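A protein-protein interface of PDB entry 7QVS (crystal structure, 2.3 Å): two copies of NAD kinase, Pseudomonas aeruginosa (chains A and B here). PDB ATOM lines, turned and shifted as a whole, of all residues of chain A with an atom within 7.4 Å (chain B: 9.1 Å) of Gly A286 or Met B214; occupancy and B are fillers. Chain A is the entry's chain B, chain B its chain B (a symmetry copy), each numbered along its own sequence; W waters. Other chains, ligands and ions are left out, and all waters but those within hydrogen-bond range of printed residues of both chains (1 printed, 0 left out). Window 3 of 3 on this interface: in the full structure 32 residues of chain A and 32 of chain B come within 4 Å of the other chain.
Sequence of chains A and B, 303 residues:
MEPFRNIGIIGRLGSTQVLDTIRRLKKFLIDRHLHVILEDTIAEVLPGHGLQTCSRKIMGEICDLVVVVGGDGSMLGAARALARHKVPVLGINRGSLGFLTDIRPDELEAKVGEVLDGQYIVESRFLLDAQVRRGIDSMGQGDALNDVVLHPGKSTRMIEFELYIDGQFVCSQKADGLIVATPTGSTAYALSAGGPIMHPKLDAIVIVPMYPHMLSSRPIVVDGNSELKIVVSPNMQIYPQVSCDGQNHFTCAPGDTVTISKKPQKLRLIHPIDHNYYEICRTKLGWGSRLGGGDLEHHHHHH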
ATOM      1  N   ILE A 280     -10.914  23.636 -19.306  1.00  0.00           N
ATOM      2  CA  ILE A 280      -9.935  23.079 -20.236  1.00  0.00           C
ATOM      3  C   ILE A 280     -10.568  22.813 -21.595  1.00  0.00           C
ATOM      4  O   ILE A 280      -9.975  23.114 -22.633  1.00  0.00           O
ATOM      5  CB  ILE A 280      -9.312  21.804 -19.635  1.00  0.00           C
ATOM      6  CG1 ILE A 280      -8.655  22.130 -18.294  1.00  0.00           C
ATOM      7  CG2 ILE A 280      -8.317  21.165 -20.583  1.00  0.00           C
ATOM      8  CD1 ILE A 280      -8.147  20.907 -17.587  1.00  0.00           C
ATOM      9  N   CYS A 281     -11.781  22.247 -21.613  1.00  0.00           N
ATOM     10  CA  CYS A 281     -12.468  22.013 -22.885  1.00  0.00           C
ATOM     11  C   CYS A 281     -12.732  23.316 -23.624  1.00  0.00           C
ATOM     12  O   CYS A 281     -12.560  23.383 -24.846  1.00  0.00           O
ATOM     13  CB  CYS A 281     -13.793  21.285 -22.663  1.00  0.00           C
ATOM     14  SG  CYS A 281     -13.653  19.603 -22.118  1.00  0.00           S
ATOM     15  N   ARG A 282     -13.161  24.358 -22.896  1.00  0.00           N
ATOM     16  CA  ARG A 282     -13.457  25.645 -23.521  1.00  0.00           C
ATOM     17  C   ARG A 282     -12.209  26.273 -24.124  1.00  0.00           C
ATOM     18  O   ARG A 282     -12.265  26.819 -25.229  1.00  0.00           O
ATOM     19  CB  ARG A 282     -14.070  26.616 -22.507  1.00  0.00           C
ATOM     20  CG  ARG A 282     -15.523  26.366 -22.142  1.00  0.00           C
ATOM     21  CD  ARG A 282     -16.149  27.590 -21.439  1.00  0.00           C
ATOM     22  NE  ARG A 282     -15.564  27.886 -20.132  1.00  0.00           N
ATOM     23  CZ  ARG A 282     -15.696  27.118 -19.054  1.00  0.00           C
ATOM     24  NH1 ARG A 282     -16.364  25.973 -19.094  1.00  0.00           N
ATOM     25  NH2 ARG A 282     -15.161  27.518 -17.902  1.00  0.00           N
ATOM     26  N   THR A 283     -11.074  26.236 -23.415  1.00  0.00           N
ATOM     27  CA  THR A 283      -9.914  26.943 -23.955  1.00  0.00           C
ATOM     28  C   THR A 283      -9.222  26.122 -25.040  1.00  0.00           C
ATOM     29  O   THR A 283      -8.754  26.677 -26.039  1.00  0.00           O
ATOM     30  CB  THR A 283      -8.931  27.338 -22.835  1.00  0.00           C
ATOM     31  OG1 THR A 283      -8.496  26.179 -22.131  1.00  0.00           O
ATOM     32  CG2 THR A 283      -9.604  28.258 -21.830  1.00  0.00           C
ATOM     33  N   LYS A 284      -9.182  24.805 -24.902  1.00  0.00           N
ATOM     34  CA  LYS A 284      -8.525  23.998 -25.924  1.00  0.00           C
ATOM     35  C   LYS A 284      -9.374  23.904 -27.190  1.00  0.00           C
ATOM     36  O   LYS A 284      -8.854  24.014 -28.307  1.00  0.00           O
ATOM     37  CB  LYS A 284      -8.235  22.609 -25.373  1.00  0.00           C
ATOM     38  CG  LYS A 284      -7.143  22.575 -24.325  1.00  0.00           C
ATOM     39  CD  LYS A 284      -6.355  21.282 -24.437  1.00  0.00           C
ATOM     40  CE  LYS A 284      -5.293  21.379 -25.513  1.00  0.00           C
ATOM     41  NZ  LYS A 284      -4.735  22.761 -25.607  1.00  0.00           N
ATOM     42  N   LEU A 285     -10.676  23.698 -27.044  1.00  0.00           N
ATOM     43  CA  LEU A 285     -11.542  23.486 -28.188  1.00  0.00           C
ATOM     44  C   LEU A 285     -12.241  24.758 -28.650  1.00  0.00           C
ATOM     45  O   LEU A 285     -12.922  24.730 -29.668  1.00  0.00           O
ATOM     46  CB  LEU A 285     -12.571  22.387 -27.873  1.00  0.00           C
ATOM     47  CG  LEU A 285     -11.936  21.090 -27.344  1.00  0.00           C
ATOM     48  CD1 LEU A 285     -12.974  20.096 -26.886  1.00  0.00           C
ATOM     49  CD2 LEU A 285     -11.055  20.458 -28.406  1.00  0.00           C
ATOM     50  N   GLY A 286     -12.080  25.874 -27.937  1.00  0.00           N
ATOM     51  CA  GLY A 286     -12.686  27.122 -28.360  1.00  0.00           C
ATOM     52  C   GLY A 286     -14.174  27.271 -28.100  1.00  0.00           C
ATOM     53  O   GLY A 286     -14.801  28.144 -28.699  1.00  0.00           O
ATOM     54  N   TRP A 287     -14.756  26.455 -27.227  1.00  0.00           N
ATOM     55  CA  TRP A 287     -16.183  26.545 -26.931  1.00  0.00           C
ATOM     56  C   TRP A 287     -16.526  27.882 -26.281  1.00  0.00           C
ATOM     57  O   TRP A 287     -15.697  28.505 -25.611  1.00  0.00           O
ATOM     58  CB  TRP A 287     -16.615  25.409 -26.001  1.00  0.00           C
ATOM     59  CG  TRP A 287     -16.523  24.048 -26.595  1.00  0.00           C
ATOM     60  CD1 TRP A 287     -16.226  23.728 -27.894  1.00  0.00           C
ATOM     61  CD2 TRP A 287     -16.731  22.808 -25.911  1.00  0.00           C
ATOM     62  NE1 TRP A 287     -16.242  22.366 -28.053  1.00  0.00           N
ATOM     63  CE2 TRP A 287     -16.550  21.779 -26.852  1.00  0.00           C
ATOM     64  CE3 TRP A 287     -17.050  22.467 -24.588  1.00  0.00           C
ATOM     65  CZ2 TRP A 287     -16.683  20.434 -26.515  1.00  0.00           C
ATOM     66  CZ3 TRP A 287     -17.187  21.127 -24.261  1.00  0.00           C
ATOM     67  CH2 TRP A 287     -17.006  20.133 -25.218  1.00  0.00           C
ATOM     68  N   GLY A 288     -17.786  28.291 -26.447  1.00  0.00           N
ATOM     69  CA  GLY A 288     -18.210  29.592 -25.951  1.00  0.00           C
ATOM     70  C   GLY A 288     -18.142  29.695 -24.433  1.00  0.00           C
ATOM     71  O   GLY A 288     -18.374  28.728 -23.707  1.00  0.00           O
ATOM     72  N   SER A 289     -17.821  30.891 -23.954  1.00  0.00           N
ATOM     73  CA  SER A 289     -17.816  31.183 -22.533  1.00  0.00           C
ATOM     74  C   SER A 289     -19.195  31.705 -22.099  1.00  0.00           C
ATOM     75  O   SER A 289     -20.146  31.716 -22.880  1.00  0.00           O
ATOM     76  CB  SER A 289     -16.699  32.174 -22.224  1.00  0.00           C
ATOM     77  OG  SER A 289     -16.956  33.397 -22.885  1.00  0.00           O
ATOM     78  N   MET B 158     -31.064  30.440 -35.552  1.00  0.00           N
ATOM     79  CA  MET B 158     -30.327  29.737 -34.517  1.00  0.00           C
ATOM     80  C   MET B 158     -30.721  30.267 -33.142  1.00  0.00           C
ATOM     81  O   MET B 158     -31.112  31.423 -32.976  1.00  0.00           O
ATOM     82  CB  MET B 158     -28.821  29.872 -34.736  1.00  0.00           C
ATOM     83  CG  MET B 158     -28.269  28.990 -35.874  1.00  0.00           C
ATOM     84  SD  MET B 158     -26.464  28.959 -35.968  1.00  0.00           S
ATOM     85  CE  MET B 158     -26.169  30.606 -36.585  1.00  0.00           C
ATOM     86  N   VAL B 170     -20.319  24.392 -18.485  1.00  0.00           N
ATOM     87  CA  VAL B 170     -19.619  23.692 -19.554  1.00  0.00           C
ATOM     88  C   VAL B 170     -19.290  24.684 -20.659  1.00  0.00           C
ATOM     89  O   VAL B 170     -18.116  24.951 -20.925  1.00  0.00           O
ATOM     90  CB  VAL B 170     -20.447  22.511 -20.092  1.00  0.00           C
ATOM     91  CG1 VAL B 170     -19.756  21.870 -21.300  1.00  0.00           C
ATOM     92  CG2 VAL B 170     -20.694  21.500 -18.981  1.00  0.00           C
ATOM     93  N   CYS B 171     -20.316  25.259 -21.284  1.00  0.00           N
ATOM     94  CA  CYS B 171     -20.121  26.213 -22.369  1.00  0.00           C
ATOM     95  C   CYS B 171     -21.452  26.841 -22.751  1.00  0.00           C
ATOM     96  O   CYS B 171     -22.527  26.341 -22.410  1.00  0.00           O
ATOM     97  CB  CYS B 171     -19.485  25.546 -23.605  1.00  0.00           C
ATOM     98  SG  CYS B 171     -20.572  24.388 -24.483  1.00  0.00           S
ATOM     99  N   SER B 172     -21.357  27.939 -23.475  1.00  0.00           N
ATOM    100  CA  SER B 172     -22.474  28.474 -24.232  1.00  0.00           C
ATOM    101  C   SER B 172     -22.280  28.109 -25.693  1.00  0.00           C
ATOM    102  O   SER B 172     -21.165  27.835 -26.132  1.00  0.00           O
ATOM    103  CB  SER B 172     -22.566  29.990 -24.089  1.00  0.00           C
ATOM    104  OG  SER B 172     -21.530  30.595 -24.834  1.00  0.00           O
ATOM    105  N   GLN B 173     -23.369  28.137 -26.454  1.00  0.00           N
ATOM    106  CA  GLN B 173     -23.200  27.978 -27.890  1.00  0.00           C
ATOM    107  C   GLN B 173     -24.427  28.454 -28.643  1.00  0.00           C
ATOM    108  O   GLN B 173     -25.515  28.606 -28.091  1.00  0.00           O
ATOM    109  CB  GLN B 173     -22.890  26.531 -28.264  1.00  0.00           C
ATOM    110  CG  GLN B 173     -24.067  25.633 -28.167  1.00  0.00           C
ATOM    111  CD  GLN B 173     -23.659  24.179 -28.230  1.00  0.00           C
ATOM    112  OE1 GLN B 173     -23.903  23.428 -27.286  1.00  0.00           O
ATOM    113  NE2 GLN B 173     -23.058  23.765 -29.351  1.00  0.00           N
ATOM    114  N   LYS B 174     -24.191  28.738 -29.914  1.00  0.00           N
ATOM    115  CA  LYS B 174     -25.208  29.047 -30.902  1.00  0.00           C
ATOM    116  C   LYS B 174     -25.388  27.805 -31.763  1.00  0.00           C
ATOM    117  O   LYS B 174     -24.404  27.264 -32.278  1.00  0.00           O
ATOM    118  CB  LYS B 174     -24.775  30.227 -31.773  1.00  0.00           C
ATOM    119  CG  LYS B 174     -25.764  31.334 -31.946  1.00  0.00           C
ATOM    120  CD  LYS B 174     -25.096  32.565 -32.581  1.00  0.00           C
ATOM    121  CE  LYS B 174     -25.947  33.108 -33.738  1.00  0.00           C
ATOM    122  NZ  LYS B 174     -25.302  34.214 -34.519  1.00  0.00           N
ATOM    123  N   ALA B 175     -26.629  27.355 -31.909  1.00  0.00           N
ATOM    124  CA  ALA B 175     -26.949  26.124 -32.632  1.00  0.00           C
ATOM    125  C   ALA B 175     -28.456  26.097 -32.878  1.00  0.00           C
ATOM    126  O   ALA B 175     -29.195  26.967 -32.403  1.00  0.00           O
ATOM    127  CB  ALA B 175     -26.483  24.894 -31.853  1.00  0.00           C
ATOM    128  N   ASP B 176     -28.909  25.089 -33.636  1.00  0.00           N
ATOM    129  CA  ASP B 176     -30.347  24.831 -33.705  1.00  0.00           C
ATOM    130  C   ASP B 176     -30.893  24.384 -32.346  1.00  0.00           C
ATOM    131  O   ASP B 176     -32.066  24.619 -32.041  1.00  0.00           O
ATOM    132  CB  ASP B 176     -30.659  23.766 -34.746  1.00  0.00           C
ATOM    133  CG  ASP B 176     -30.914  24.346 -36.157  1.00  0.00           C
ATOM    134  OD1 ASP B 176     -30.566  25.515 -36.447  1.00  0.00           O
ATOM    135  OD2 ASP B 176     -31.469  23.595 -36.987  1.00  0.00           O
ATOM    136  N   PRO B 209     -24.958  18.337 -29.835  1.00  0.00           N
ATOM    137  CA  PRO B 209     -25.411  19.626 -30.376  1.00  0.00           C
ATOM    138  C   PRO B 209     -26.049  19.447 -31.750  1.00  0.00           C
ATOM    139  O   PRO B 209     -25.584  18.646 -32.560  1.00  0.00           O
ATOM    140  CB  PRO B 209     -24.119  20.455 -30.456  1.00  0.00           C
ATOM    141  CG  PRO B 209     -23.104  19.705 -29.673  1.00  0.00           C
ATOM    142  CD  PRO B 209     -23.495  18.243 -29.764  1.00  0.00           C
ATOM    143  N   MET B 210     -27.131  20.190 -32.001  1.00  0.00           N
ATOM    144  CA  MET B 210     -27.849  20.153 -33.272  1.00  0.00           C
ATOM    145  C   MET B 210     -27.407  21.310 -34.152  1.00  0.00           C
ATOM    146  O   MET B 210     -27.683  22.473 -33.822  1.00  0.00           O
ATOM    147  CB  MET B 210     -29.354  20.274 -33.084  1.00  0.00           C
ATOM    148  CG  MET B 210     -30.012  19.258 -32.233  1.00  0.00           C
ATOM    149  SD  MET B 210     -31.805  19.539 -32.225  1.00  0.00           S
ATOM    150  CE  MET B 210     -32.161  20.432 -33.725  1.00  0.00           C
ATOM    151  N   TYR B 211     -26.813  20.989 -35.299  1.00  0.00           N
ATOM    152  CA  TYR B 211     -26.375  21.972 -36.283  1.00  0.00           C
ATOM    153  C   TYR B 211     -25.629  23.136 -35.622  1.00  0.00           C
ATOM    154  O   TYR B 211     -26.072  24.286 -35.695  1.00  0.00           O
ATOM    155  CB  TYR B 211     -27.563  22.493 -37.092  1.00  0.00           C
ATOM    156  CG  TYR B 211     -28.409  21.407 -37.699  1.00  0.00           C
ATOM    157  CD1 TYR B 211     -27.983  20.700 -38.834  1.00  0.00           C
ATOM    158  CD2 TYR B 211     -29.622  21.050 -37.113  1.00  0.00           C
ATOM    159  CE1 TYR B 211     -28.762  19.679 -39.373  1.00  0.00           C
ATOM    160  CE2 TYR B 211     -30.404  20.038 -37.639  1.00  0.00           C
ATOM    161  CZ  TYR B 211     -29.977  19.359 -38.768  1.00  0.00           C
ATOM    162  OH  TYR B 211     -30.779  18.354 -39.248  1.00  0.00           O
ATOM    163  N   PRO B 212     -24.529  22.862 -34.924  1.00  0.00           N
ATOM    164  CA  PRO B 212     -23.855  23.935 -34.177  1.00  0.00           C
ATOM    165  C   PRO B 212     -23.138  24.910 -35.099  1.00  0.00           C
ATOM    166  O   PRO B 212     -22.591  24.537 -36.140  1.00  0.00           O
ATOM    167  CB  PRO B 212     -22.857  23.183 -33.291  1.00  0.00           C
ATOM    168  CG  PRO B 212     -22.587  21.904 -34.040  1.00  0.00           C
ATOM    169  CD  PRO B 212     -23.880  21.552 -34.732  1.00  0.00           C
ATOM    170  N   HIS B 213     -23.171  26.175 -34.701  1.00  0.00           N
ATOM    171  CA  HIS B 213     -22.372  27.220 -35.340  1.00  0.00           C
ATOM    172  C   HIS B 213     -20.874  26.938 -35.208  1.00  0.00           C
ATOM    173  O   HIS B 213     -20.097  27.140 -36.158  1.00  0.00           O
ATOM    174  CB  HIS B 213     -22.734  28.565 -34.686  1.00  0.00           C
ATOM    175  CG  HIS B 213     -22.322  29.774 -35.464  1.00  0.00           C
ATOM    176  ND1 HIS B 213     -22.797  30.051 -36.730  1.00  0.00           N
ATOM    177  CD2 HIS B 213     -21.520  30.810 -35.126  1.00  0.00           C
ATOM    178  CE1 HIS B 213     -22.289  31.198 -37.145  1.00  0.00           C
ATOM    179  NE2 HIS B 213     -21.511  31.680 -36.191  1.00  0.00           N
ATOM    180  N   MET B 214     -20.442  26.502 -34.029  1.00  0.00           N
ATOM    181  CA  MET B 214     -19.023  26.279 -33.796  1.00  0.00           C
ATOM    182  C   MET B 214     -18.634  24.909 -34.327  1.00  0.00           C
ATOM    183  O   MET B 214     -19.190  23.902 -33.899  1.00  0.00           O
ATOM    184  CB  MET B 214     -18.709  26.393 -32.309  1.00  0.00           C
ATOM    185  CG  MET B 214     -17.335  25.882 -31.951  1.00  0.00           C
ATOM    186  SD  MET B 214     -16.583  27.060 -30.840  1.00  0.00           S
ATOM    187  CE  MET B 214     -16.338  28.411 -31.992  1.00  0.00           C
ATOM    188  N   LEU B 215     -17.666  24.871 -35.237  1.00  0.00           N
ATOM    189  CA  LEU B 215     -17.314  23.611 -35.877  1.00  0.00           C
ATOM    190  C   LEU B 215     -16.659  22.632 -34.898  1.00  0.00           C
ATOM    191  O   LEU B 215     -16.819  21.418 -35.051  1.00  0.00           O
ATOM    192  CB  LEU B 215     -16.417  23.889 -37.081  1.00  0.00           C
ATOM    193  CG  LEU B 215     -17.083  24.685 -38.218  1.00  0.00           C
ATOM    194  CD1 LEU B 215     -16.108  25.028 -39.331  1.00  0.00           C
ATOM    195  CD2 LEU B 215     -18.275  23.936 -38.782  1.00  0.00           C
ATOM    196  N   SER B 216     -15.956  23.124 -33.871  1.00  0.00           N
ATOM    197  CA  SER B 216     -15.350  22.242 -32.867  1.00  0.00           C
ATOM    198  C   SER B 216     -16.337  21.740 -31.821  1.00  0.00           C
ATOM    199  O   SER B 216     -15.917  21.084 -30.867  1.00  0.00           O
ATOM    200  CB  SER B 216     -14.191  22.952 -32.156  1.00  0.00           C
ATOM    201  OG  SER B 216     -14.667  24.045 -31.390  1.00  0.00           O
ATOM    202  N   SER B 217     -17.621  22.051 -31.953  1.00  0.00           N
ATOM    203  CA  SER B 217     -18.629  21.416 -31.127  1.00  0.00           C
ATOM    204  C   SER B 217     -18.590  19.917 -31.366  1.00  0.00           C
ATOM    205  O   SER B 217     -18.439  19.472 -32.507  1.00  0.00           O
ATOM    206  CB  SER B 217     -20.013  21.966 -31.468  1.00  0.00           C
ATOM    207  OG  SER B 217     -20.554  22.714 -30.398  1.00  0.00           O
ATOM    208  N   ARG B 218     -18.683  19.139 -30.289  1.00  0.00           N
ATOM    209  CA  ARG B 218     -18.613  17.689 -30.400  1.00  0.00           C
ATOM    210  C   ARG B 218     -19.484  17.097 -29.311  1.00  0.00           C
ATOM    211  O   ARG B 218     -19.682  17.728 -28.270  1.00  0.00           O
ATOM    212  CB  ARG B 218     -17.172  17.153 -30.296  1.00  0.00           C
ATOM    213  CG  ARG B 218     -16.305  17.413 -31.538  1.00  0.00           C
ATOM    214  CD  ARG B 218     -16.945  16.847 -32.826  1.00  0.00           C
ATOM    215  NE  ARG B 218     -15.993  16.834 -33.936  1.00  0.00           N
ATOM    216  CZ  ARG B 218     -15.667  17.904 -34.653  1.00  0.00           C
ATOM    217  NH1 ARG B 218     -16.210  19.093 -34.414  1.00  0.00           N
ATOM    218  NH2 ARG B 218     -14.763  17.786 -35.624  1.00  0.00           N
HETATM  219  O   HOH W   1     -19.601  26.967 -28.312  1.00  0.00           O
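Trp A287 touches Val B170.
Cys B171 touches Trp A287 (CB to CB, 3.7 Å).
Trp A287 touches Met B214.
O of Gly A288 touches CA of Cys B171, at 3.3 Å.
O of Val B170 is in hydrogen-bond range of NH1 of Arg A282 (2.7 Å).
O of Leu A285 sits at hydrogen-bond distance from OG of Ser B216 (2.5 Å).
The indole nitrogen of Trp A287 lies within hydrogen-bond range of the backbone carbonyl oxygen of Ser B216.
The backbone carbonyl oxygen (O) of Gly A288 is in hydrogen-bond range of the backbone NH (N) of Ser B172.
OG of Ser B172 lies within hydrogen-bond range of O of Ser A289, 2.6 Å away.
SD of Met B214 lies close to O of Gly A286 (3.0 Å).
Met B214 touches two residues of chain A.
Of the printed residues of chain A, Val B170 touches Arg A282 and Trp A287.
Of the printed residues of chain B, Gly A288 touches Cys B171 and Ser B172.
Of the printed residues of chain A, Ser B172 touches Gly A288 and Ser A289.
Of the printed residues of chain B, Leu A285 touches Ser B216 (2.5 Å).
Asp B176 touches none of the printed residues of chain A.
Tyr B211 touches none of the printed residues of chain A.
The nearest residue of chain A that does not touch Met B214 is Leu A285 (4.5 Å).
The nearest printed residue of chain A that does not touch Ser B216 is Gly A286 (4.6 Å).
Water W1 bridges the backbone carbonyl oxygen of Ser B172 (2.8 Å) and the backbone NH of Gly A288 (2.9 Å).
The backbone carbonyl oxygen of Arg A282 lies within hydrogen-bond range of the backbone NH of Trp A287.
The side-chain hydroxyl of Ser B216 sits close to the side-chain sulfur of Met B214 (3.6 Å).
Hydrophobic or aromatic side chains of chain B that line the printed part of chain A: Val B170 and Met B214.
Among the printed residues, 10 pairs touch across the chains.
No position is printed for both chains.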
